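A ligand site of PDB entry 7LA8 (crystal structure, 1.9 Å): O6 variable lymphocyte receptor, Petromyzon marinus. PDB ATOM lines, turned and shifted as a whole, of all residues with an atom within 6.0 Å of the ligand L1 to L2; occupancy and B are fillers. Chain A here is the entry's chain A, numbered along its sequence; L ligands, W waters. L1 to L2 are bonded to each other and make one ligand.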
ATOM      1  N   ASN A  15      13.742  -5.837  27.771  1.00  0.00           N
ATOM      2  CA  ASN A  15      14.822  -5.081  28.334  1.00  0.00           C
ATOM      3  C   ASN A  15      15.962  -6.032  28.688  1.00  0.00           C
ATOM      4  O   ASN A  15      15.944  -6.704  29.739  1.00  0.00           O
ATOM      5  CB  ASN A  15      14.319  -4.327  29.551  1.00  0.00           C
ATOM      6  CG  ASN A  15      15.461  -3.673  30.293  1.00  0.00           C
ATOM      7  OD1 ASN A  15      16.602  -3.648  29.798  1.00  0.00           O
ATOM      8  ND2 ASN A  15      15.170  -3.170  31.471  1.00  0.00           N
ATOM      9  N   ASP A  17      19.085  -4.678  28.870  1.00  0.00           N
ATOM     10  CA  ASP A  17      20.104  -3.694  29.229  1.00  0.00           C
ATOM     11  C   ASP A  17      20.965  -4.255  30.371  1.00  0.00           C
ATOM     12  O   ASP A  17      20.444  -4.546  31.449  1.00  0.00           O
ATOM     13  CB  ASP A  17      19.371  -2.391  29.640  1.00  0.00           C
ATOM     14  CG  ASP A  17      20.293  -1.159  29.773  1.00  0.00           C
ATOM     15  OD1 ASP A  17      21.401  -1.166  29.250  1.00  0.00           O
ATOM     16  OD2 ASP A  17      19.871  -0.176  30.441  1.00  0.00           O
ATOM     17  N   TRP A  36      15.806  -3.184  24.321  1.00  0.00           N
ATOM     18  CA  TRP A  36      17.069  -2.692  24.879  1.00  0.00           C
ATOM     19  C   TRP A  36      18.054  -3.834  24.728  1.00  0.00           C
ATOM     20  O   TRP A  36      17.854  -4.909  25.318  1.00  0.00           O
ATOM     21  CB  TRP A  36      16.921  -2.266  26.336  1.00  0.00           C
ATOM     22  CG  TRP A  36      16.342  -0.924  26.615  1.00  0.00           C
ATOM     23  CD1 TRP A  36      17.023   0.216  26.866  1.00  0.00           C
ATOM     24  CD2 TRP A  36      14.950  -0.601  26.744  1.00  0.00           C
ATOM     25  NE1 TRP A  36      16.157   1.242  27.145  1.00  0.00           N
ATOM     26  CE2 TRP A  36      14.870   0.752  27.051  1.00  0.00           C
ATOM     27  CE3 TRP A  36      13.764  -1.336  26.594  1.00  0.00           C
ATOM     28  CZ2 TRP A  36      13.661   1.399  27.208  1.00  0.00           C
ATOM     29  CZ3 TRP A  36      12.592  -0.711  26.770  1.00  0.00           C
ATOM     30  CH2 TRP A  36      12.534   0.640  27.081  1.00  0.00           C
ATOM     31  N   SER A  38      21.272  -2.670  24.972  1.00  0.00           N
ATOM     32  CA  SER A  38      22.387  -1.833  25.367  1.00  0.00           C
ATOM     33  C   SER A  38      23.144  -2.427  26.554  1.00  0.00           C
ATOM     34  O   SER A  38      22.648  -3.309  27.264  1.00  0.00           O
ATOM     35  CB  SER A  38      21.902  -0.431  25.730  1.00  0.00           C
ATOM     36  OG  SER A  38      20.655  -0.459  26.400  1.00  0.00           O
ATOM     37  N   ASN A  39      24.375  -1.913  26.746  1.00  0.00           N
ATOM     38  CA  ASN A  39      25.242  -2.336  27.867  1.00  0.00           C
ATOM     39  C   ASN A  39      25.448  -3.843  27.913  1.00  0.00           C
ATOM     40  O   ASN A  39      25.327  -4.490  28.934  1.00  0.00           O
ATOM     41  CB  ASN A  39      24.688  -1.821  29.166  1.00  0.00           C
ATOM     42  CG  ASN A  39      24.845  -0.329  29.308  1.00  0.00           C
ATOM     43  OD1 ASN A  39      25.957   0.187  29.316  1.00  0.00           O
ATOM     44  ND2 ASN A  39      23.739   0.352  29.454  1.00  0.00           N
ATOM     45  N   TYR A  60      17.702  -0.010  21.142  1.00  0.00           N
ATOM     46  CA  TYR A  60      18.859   0.575  21.827  1.00  0.00           C
ATOM     47  C   TYR A  60      20.002  -0.432  21.779  1.00  0.00           C
ATOM     48  O   TYR A  60      19.911  -1.518  22.362  1.00  0.00           O
ATOM     49  CB  TYR A  60      18.503   1.007  23.249  1.00  0.00           C
ATOM     50  CG  TYR A  60      17.273   1.935  23.283  1.00  0.00           C
ATOM     51  CD1 TYR A  60      16.085   1.520  23.867  1.00  0.00           C
ATOM     52  CD2 TYR A  60      17.294   3.205  22.706  1.00  0.00           C
ATOM     53  CE1 TYR A  60      14.964   2.337  23.921  1.00  0.00           C
ATOM     54  CE2 TYR A  60      16.163   4.056  22.749  1.00  0.00           C
ATOM     55  CZ  TYR A  60      14.989   3.574  23.342  1.00  0.00           C
ATOM     56  OH  TYR A  60      13.847   4.356  23.400  1.00  0.00           O
ATOM     57  N   LEU A  61      21.030  -0.102  21.003  1.00  0.00           N
ATOM     58  CA  LEU A  61      22.236  -0.905  20.817  1.00  0.00           C
ATOM     59  C   LEU A  61      23.462  -0.221  21.411  1.00  0.00           C
ATOM     60  O   LEU A  61      24.580  -0.703  21.247  1.00  0.00           O
ATOM     61  CB  LEU A  61      22.482  -1.192  19.301  1.00  0.00           C
ATOM     62  CG  LEU A  61      21.449  -2.137  18.672  1.00  0.00           C
ATOM     63  CD1 LEU A  61      21.488  -2.054  17.199  1.00  0.00           C
ATOM     64  CD2 LEU A  61      21.720  -3.594  19.098  1.00  0.00           C
ATOM     65  N   SER A  62      23.235   0.852  22.159  1.00  0.00           N
ATOM     66  CA  SER A  62      24.293   1.637  22.785  1.00  0.00           C
ATOM     67  C   SER A  62      25.073   0.817  23.789  1.00  0.00           C
ATOM     68  O   SER A  62      24.536  -0.082  24.442  1.00  0.00           O
ATOM     69  CB  SER A  62      23.730   2.864  23.523  1.00  0.00           C
ATOM     70  OG  SER A  62      22.502   3.319  22.948  1.00  0.00           O
ATOM     71  N   ASN A  63      26.336   1.189  23.964  1.00  0.00           N
ATOM     72  CA  ASN A  63      27.209   0.586  24.994  1.00  0.00           C
ATOM     73  C   ASN A  63      27.476  -0.890  24.726  1.00  0.00           C
ATOM     74  O   ASN A  63      27.205  -1.763  25.534  1.00  0.00           O
ATOM     75  CB  ASN A  63      26.605   0.783  26.367  1.00  0.00           C
ATOM     76  CG  ASN A  63      26.826   2.137  26.892  1.00  0.00           C
ATOM     77  OD1 ASN A  63      25.909   2.975  26.925  1.00  0.00           O
ATOM     78  ND2 ASN A  63      28.057   2.399  27.300  1.00  0.00           N
ATOM     79  N   GLY A  84      19.483   3.855  19.094  1.00  0.00           N
ATOM     80  CA  GLY A  84      20.655   4.123  19.930  1.00  0.00           C
ATOM     81  C   GLY A  84      21.858   3.357  19.377  1.00  0.00           C
ATOM     82  O   GLY A  84      21.906   2.119  19.414  1.00  0.00           O
ATOM     83  N   ASP A  86      25.123   4.940  19.989  1.00  0.00           N
ATOM     84  CA  ASP A  86      26.222   5.614  20.665  1.00  0.00           C
ATOM     85  C   ASP A  86      27.037   4.623  21.480  1.00  0.00           C
ATOM     86  O   ASP A  86      26.543   3.569  21.905  1.00  0.00           O
ATOM     87  CB  ASP A  86      25.680   6.689  21.598  1.00  0.00           C
ATOM     88  CG  ASP A  86      24.631   6.150  22.528  1.00  0.00           C
ATOM     89  OD1 ASP A  86      24.864   6.192  23.751  1.00  0.00           O
ATOM     90  OD2 ASP A  86      23.563   5.603  22.070  1.00  0.00           O
ATOM     91  N   GLN A  87      28.275   5.019  21.767  1.00  0.00           N
ATOM     92  CA  GLN A  87      29.150   4.282  22.658  1.00  0.00           C
ATOM     93  C   GLN A  87      29.365   2.867  22.134  1.00  0.00           C
ATOM     94  O   GLN A  87      28.999   1.877  22.770  1.00  0.00           O
ATOM     95  CB  GLN A  87      28.604   4.270  24.091  1.00  0.00           C
ATOM     96  CG  GLN A  87      28.252   5.659  24.581  1.00  0.00           C
ATOM     97  CD  GLN A  87      27.702   5.741  26.006  1.00  0.00           C
ATOM     98  OE1 GLN A  87      28.441   5.531  26.970  1.00  0.00           O
ATOM     99  NE2 GLN A  87      26.429   6.103  26.139  1.00  0.00           N
ATOM    100  N   TRP A 108      20.936   8.397  18.482  1.00  0.00           N
ATOM    101  CA  TRP A 108      22.190   8.569  19.197  1.00  0.00           C
ATOM    102  C   TRP A 108      23.283   7.947  18.354  1.00  0.00           C
ATOM    103  O   TRP A 108      23.237   6.729  18.078  1.00  0.00           O
ATOM    104  CB  TRP A 108      22.176   7.878  20.557  1.00  0.00           C
ATOM    105  CG  TRP A 108      21.213   8.359  21.596  1.00  0.00           C
ATOM    106  CD1 TRP A 108      21.509   9.085  22.715  1.00  0.00           C
ATOM    107  CD2 TRP A 108      19.799   8.076  21.680  1.00  0.00           C
ATOM    108  NE1 TRP A 108      20.412   9.289  23.460  1.00  0.00           N
ATOM    109  CE2 TRP A 108      19.332   8.695  22.861  1.00  0.00           C
ATOM    110  CE3 TRP A 108      18.878   7.382  20.875  1.00  0.00           C
ATOM    111  CZ2 TRP A 108      17.994   8.636  23.275  1.00  0.00           C
ATOM    112  CZ3 TRP A 108      17.539   7.339  21.272  1.00  0.00           C
ATOM    113  CH2 TRP A 108      17.114   7.952  22.470  1.00  0.00           C
ATOM    114  N   HIS A 110      26.774   9.368  19.009  1.00  0.00           N
ATOM    115  CA  HIS A 110      28.019   9.873  19.569  1.00  0.00           C
ATOM    116  C   HIS A 110      28.871   8.753  20.176  1.00  0.00           C
ATOM    117  O   HIS A 110      28.440   7.623  20.376  1.00  0.00           O
ATOM    118  CB  HIS A 110      27.759  10.911  20.657  1.00  0.00           C
ATOM    119  CG  HIS A 110      27.040  10.374  21.854  1.00  0.00           C
ATOM    120  ND1 HIS A 110      27.670   9.661  22.862  1.00  0.00           N
ATOM    121  CD2 HIS A 110      25.726  10.438  22.210  1.00  0.00           C
ATOM    122  CE1 HIS A 110      26.769   9.322  23.778  1.00  0.00           C
ATOM    123  NE2 HIS A 110      25.582   9.767  23.392  1.00  0.00           N
ATOM    124  N   THR A 111      30.096   9.119  20.537  1.00  0.00           N
ATOM    125  CA  THR A 111      31.059   8.227  21.165  1.00  0.00           C
ATOM    126  C   THR A 111      31.271   6.978  20.313  1.00  0.00           C
ATOM    127  O   THR A 111      31.212   5.839  20.772  1.00  0.00           O
ATOM    128  CB  THR A 111      30.662   7.901  22.621  1.00  0.00           C
ATOM    129  OG1 THR A 111      30.372   9.107  23.323  1.00  0.00           O
ATOM    130  CG2 THR A 111      31.776   7.252  23.371  1.00  0.00           C
ATOM    131  N   GLY A 136      21.204  13.466  18.866  1.00  0.00           N
ATOM    132  CA  GLY A 136      21.364  14.025  20.189  1.00  0.00           C
ATOM    133  C   GLY A 136      21.996  13.111  21.208  1.00  0.00           C
ATOM    134  O   GLY A 136      22.754  12.195  20.876  1.00  0.00           O
ATOM    135  N   GLU A 137      21.645  13.371  22.466  1.00  0.00           N
ATOM    136  CA  GLU A 137      22.222  12.692  23.620  1.00  0.00           C
ATOM    137  C   GLU A 137      21.290  12.838  24.817  1.00  0.00           C
ATOM    138  O   GLU A 137      20.468  13.754  24.875  1.00  0.00           O
ATOM    139  CB  GLU A 137      23.581  13.284  23.973  1.00  0.00           C
ATOM    140  CG  GLU A 137      23.509  14.752  24.414  1.00  0.00           C
ATOM    141  CD  GLU A 137      24.866  15.460  24.333  1.00  0.00           C
ATOM    142  OE1 GLU A 137      25.165  16.374  25.179  1.00  0.00           O
ATOM    143  OE2 GLU A 137      25.640  15.175  23.402  1.00  0.00           O
ATOM    144  N   GLY A 138      21.478  11.959  25.791  1.00  0.00           N
ATOM    145  CA  GLY A 138      20.703  11.999  26.996  1.00  0.00           C
ATOM    146  C   GLY A 138      19.522  11.054  26.928  1.00  0.00           C
ATOM    147  O   GLY A 138      19.458  10.109  26.134  1.00  0.00           O
ATOM    148  N   TRP A 139      18.576  11.278  27.838  1.00  0.00           N
ATOM    149  CA  TRP A 139      17.503  10.307  28.051  1.00  0.00           C
ATOM    150  C   TRP A 139      16.370  10.997  28.793  1.00  0.00           C
ATOM    151  O   TRP A 139      16.597  11.663  29.790  1.00  0.00           O
ATOM    152  CB  TRP A 139      18.022   9.119  28.844  1.00  0.00           C
ATOM    153  CG  TRP A 139      17.026   7.963  29.031  1.00  0.00           C
ATOM    154  CD1 TRP A 139      16.449   7.569  30.200  1.00  0.00           C
ATOM    155  CD2 TRP A 139      16.559   7.067  28.022  1.00  0.00           C
ATOM    156  NE1 TRP A 139      15.646   6.470  29.987  1.00  0.00           N
ATOM    157  CE2 TRP A 139      15.701   6.132  28.657  1.00  0.00           C
ATOM    158  CE3 TRP A 139      16.783   6.944  26.664  1.00  0.00           C
ATOM    159  CZ2 TRP A 139      15.068   5.100  27.968  1.00  0.00           C
ATOM    160  CZ3 TRP A 139      16.165   5.911  25.966  1.00  0.00           C
ATOM    161  CH2 TRP A 139      15.296   5.011  26.624  1.00  0.00           C
ATOM    162  N   SER A 142      16.549  14.560  30.075  1.00  0.00           N
ATOM    163  CA  SER A 142      17.884  15.079  29.764  1.00  0.00           C
ATOM    164  C   SER A 142      18.221  14.985  28.275  1.00  0.00           C
ATOM    165  O   SER A 142      19.354  15.289  27.888  1.00  0.00           O
ATOM    166  CB  SER A 142      18.941  14.341  30.589  1.00  0.00           C
ATOM    167  OG  SER A 142      19.132  13.027  30.077  1.00  0.00           O
HETATM  168  C1  LIG L   1      17.944   3.470  31.902  1.00  0.00           C
HETATM  169  C2  LIG L   1      17.484   3.154  30.489  1.00  0.00           C
HETATM  170  C3  LIG L   1      18.628   3.412  29.531  1.00  0.00           C
HETATM  171  C4  LIG L   1      19.214   4.804  29.711  1.00  0.00           C
HETATM  172  C5  LIG L   1      19.522   5.119  31.173  1.00  0.00           C
HETATM  173  C6  LIG L   1      19.829   6.573  31.393  1.00  0.00           C
HETATM  174  C7  LIG L   1      15.791   1.324  30.518  1.00  0.00           C
HETATM  175  C8  LIG L   1      15.612  -0.153  30.486  1.00  0.00           C
HETATM  176  N1  LIG L   1      17.058   1.763  30.436  1.00  0.00           N
HETATM  177  O1  LIG L   1      16.824   3.369  32.730  1.00  0.00           O
HETATM  178  O2  LIG L   1      18.163   3.197  28.200  1.00  0.00           O
HETATM  179  O3  LIG L   1      20.480   4.949  29.036  1.00  0.00           O
HETATM  180  O4  LIG L   1      18.381   4.813  31.982  1.00  0.00           O
HETATM  181  O5  LIG L   1      20.399   6.742  32.670  1.00  0.00           O
HETATM  182  O6  LIG L   1      14.817   2.100  30.462  1.00  0.00           O
HETATM  183  C1  LG2 L   2      20.490   5.799  27.922  1.00  0.00           C
HETATM  184  C2  LG2 L   2      21.866   6.409  27.807  1.00  0.00           C
HETATM  185  C3  LG2 L   2      21.928   7.362  26.677  1.00  0.00           C
HETATM  186  C4  LG2 L   2      21.593   6.621  25.458  1.00  0.00           C
HETATM  187  C5  LG2 L   2      20.221   6.018  25.554  1.00  0.00           C
HETATM  188  C6  LG2 L   2      19.743   5.276  24.320  1.00  0.00           C
HETATM  189  O1  LG2 L   2      22.158   7.130  28.978  1.00  0.00           O
HETATM  190  O2  LG2 L   2      23.362   7.662  26.647  1.00  0.00           O
HETATM  191  O3  LG2 L   2      22.571   5.549  25.376  1.00  0.00           O
HETATM  192  O4  LG2 L   2      20.196   5.082  26.654  1.00  0.00           O
HETATM  193  O5  LG2 L   2      20.283   3.948  24.399  1.00  0.00           O
HETATM  194  S1  LG2 L   2      23.915   9.209  26.599  1.00  0.00           S
HETATM  195  O6  LG2 L   2      23.253  10.007  27.696  1.00  0.00           O
HETATM  196  O7  LG2 L   2      23.534   9.762  25.234  1.00  0.00           O
HETATM  197  O8  LG2 L   2      25.394   9.236  26.546  1.00  0.00           O
HETATM  198  C1  LG3 L   3      26.626  13.718  29.691  1.00  0.00           C
HETATM  199  O1  LG3 L   3      27.691  14.325  30.019  1.00  0.00           O
HETATM  200  O2  LG3 L   3      26.278  12.693  30.317  1.00  0.00           O
HETATM  201  C2  LG3 L   3      25.816  14.188  28.511  1.00  0.00           C
HETATM  202  C3  LG3 L   3      25.511  12.983  27.649  1.00  0.00           C
HETATM  203  C4  LG3 L   3      26.776  12.402  27.016  1.00  0.00           C
HETATM  204  C5  LG3 L   3      27.181  13.187  25.763  1.00  0.00           C
HETATM  205  C6  LG3 L   3      28.446  12.601  25.106  1.00  0.00           C
HETATM  206  S1  LG3 L   3      29.834  12.913  26.019  1.00  0.00           S
HETATM  207  C7  LG3 L   3      30.865  12.578  24.571  1.00  0.00           C
HETATM  208  C8  LG3 L   3      30.118  13.093  23.354  1.00  0.00           C
HETATM  209  N1  LG3 L   3      30.449  14.476  23.028  1.00  0.00           N
HETATM  210  C9  LG3 L   3      29.438  15.283  23.272  1.00  0.00           C
HETATM  211  O3  LG3 L   3      29.453  16.682  23.081  1.00  0.00           O
HETATM  212  N2  LG3 L   3      28.389  14.591  23.696  1.00  0.00           N
HETATM  213  C10 LG3 L   3      28.653  13.178  23.725  1.00  0.00           C
HETATM  214  O   HOH W   1      14.143   4.599  31.601  1.00  0.00           O
HETATM  215  O   HOH W   2      20.152   2.255  26.446  1.00  0.00           O
HETATM  216  O   HOH W   3      12.470   1.668  30.724  1.00  0.00           O
HETATM  217  O   HOH W   4      22.899   3.317  27.023  1.00  0.00           O
HETATM  218  O   HOH W   5      22.942   3.266  29.840  1.00  0.00           O
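The side-chain hydroxyl of Ser 62 is in hydrogen-bond range of an oxygen (O5) of LG2 L2 (2.7 Å).
A ring nitrogen (NE2) of His 110 sits at hydrogen-bond distance from an oxygen (O7) of LG2 L2, 2.8 Å away.
An oxygen (O3) of LG2 L2 sits at hydrogen-bond distance from the side-chain carboxylate of Asp 86 (2.9 Å).
NE1 of Trp 36 sits at hydrogen-bond distance from O2 of LIG L1.
The backbone NH (N) of Gly 138 is in hydrogen-bond range of an oxygen (O7) of LG2 L2 (3.1 Å).
An oxygen (O8) of LG2 L2 sits at hydrogen-bond distance from the side-chain amide nitrogen of Gln 87 (3.3 Å).
The side-chain carboxylate (OD2) of Asp 17 sits at hydrogen-bond distance from a nitrogen (N1) of LIG L1 (3.4 Å).
The side-chain carboxylate of Glu 137 lies within hydrogen-bond range of a nitrogen (N2) of LG3 L3 (2.8 Å).
OD2 of Asp 86 sits at hydrogen-bond distance from OG of Ser 62, at 2.7 Å.
O of Gly 84 sits at hydrogen-bond distance from N of Ser 62, 3.3 Å away.
The backbone NH (N) of Gln 87 lies within hydrogen-bond range of the backbone carbonyl oxygen (O) of His 110 (3.0 Å).
The side-chain carboxylate of Asp 86 sits at hydrogen-bond distance from the side-chain amide nitrogen of Gln 87, at 2.9 Å.
The backbone carbonyl oxygen (O) of Gln 87 is in hydrogen-bond range of the backbone NH (N) of Asn 63 (3.0 Å).
N of Gln 87 lies close to O of Thr 111 (3.2 Å).
The side-chain carboxylate of Asp 17 sits at hydrogen-bond distance from the side-chain amide nitrogen of Asn 39 (2.8 Å).
O of Tyr 60 is in hydrogen-bond range of N of Ser 38 (3.2 Å).
Asn 15 touches the ligand L1 to L2.
Tyr 60 touches the ligand L1 to L2.
Trp 108 touches the ligand L1 to L2.
CA of Glu 137 touches O7 of LG2 L2, at 3.6 Å.
CZ2 of Trp 139 touches O2 of LIG L1 (3.6 Å).
Hydrophobic or aromatic side chains that line the ligand L1 to L2: Trp 36, Tyr 60, Trp 108, His 110 and Trp 139.
Water W2 bridges O5 of LG2 L2 (2.7 Å) and OG of Ser 38 (2.8 Å).
Water W4 bridges O3 of LG2 L2 (2.8 Å) and OD1 of Asn 63 (3.0 Å).
Water W1 lies within hydrogen-bond range of an oxygen (O6) of LIG L1 (2.8 Å) and the indole nitrogen (NE1) of Trp 139 (2.9 Å).
Water W5 lies within hydrogen-bond range of ND2 of Asn 39 (3.0 Å) and O3 of LIG L1 (3.1 Å).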
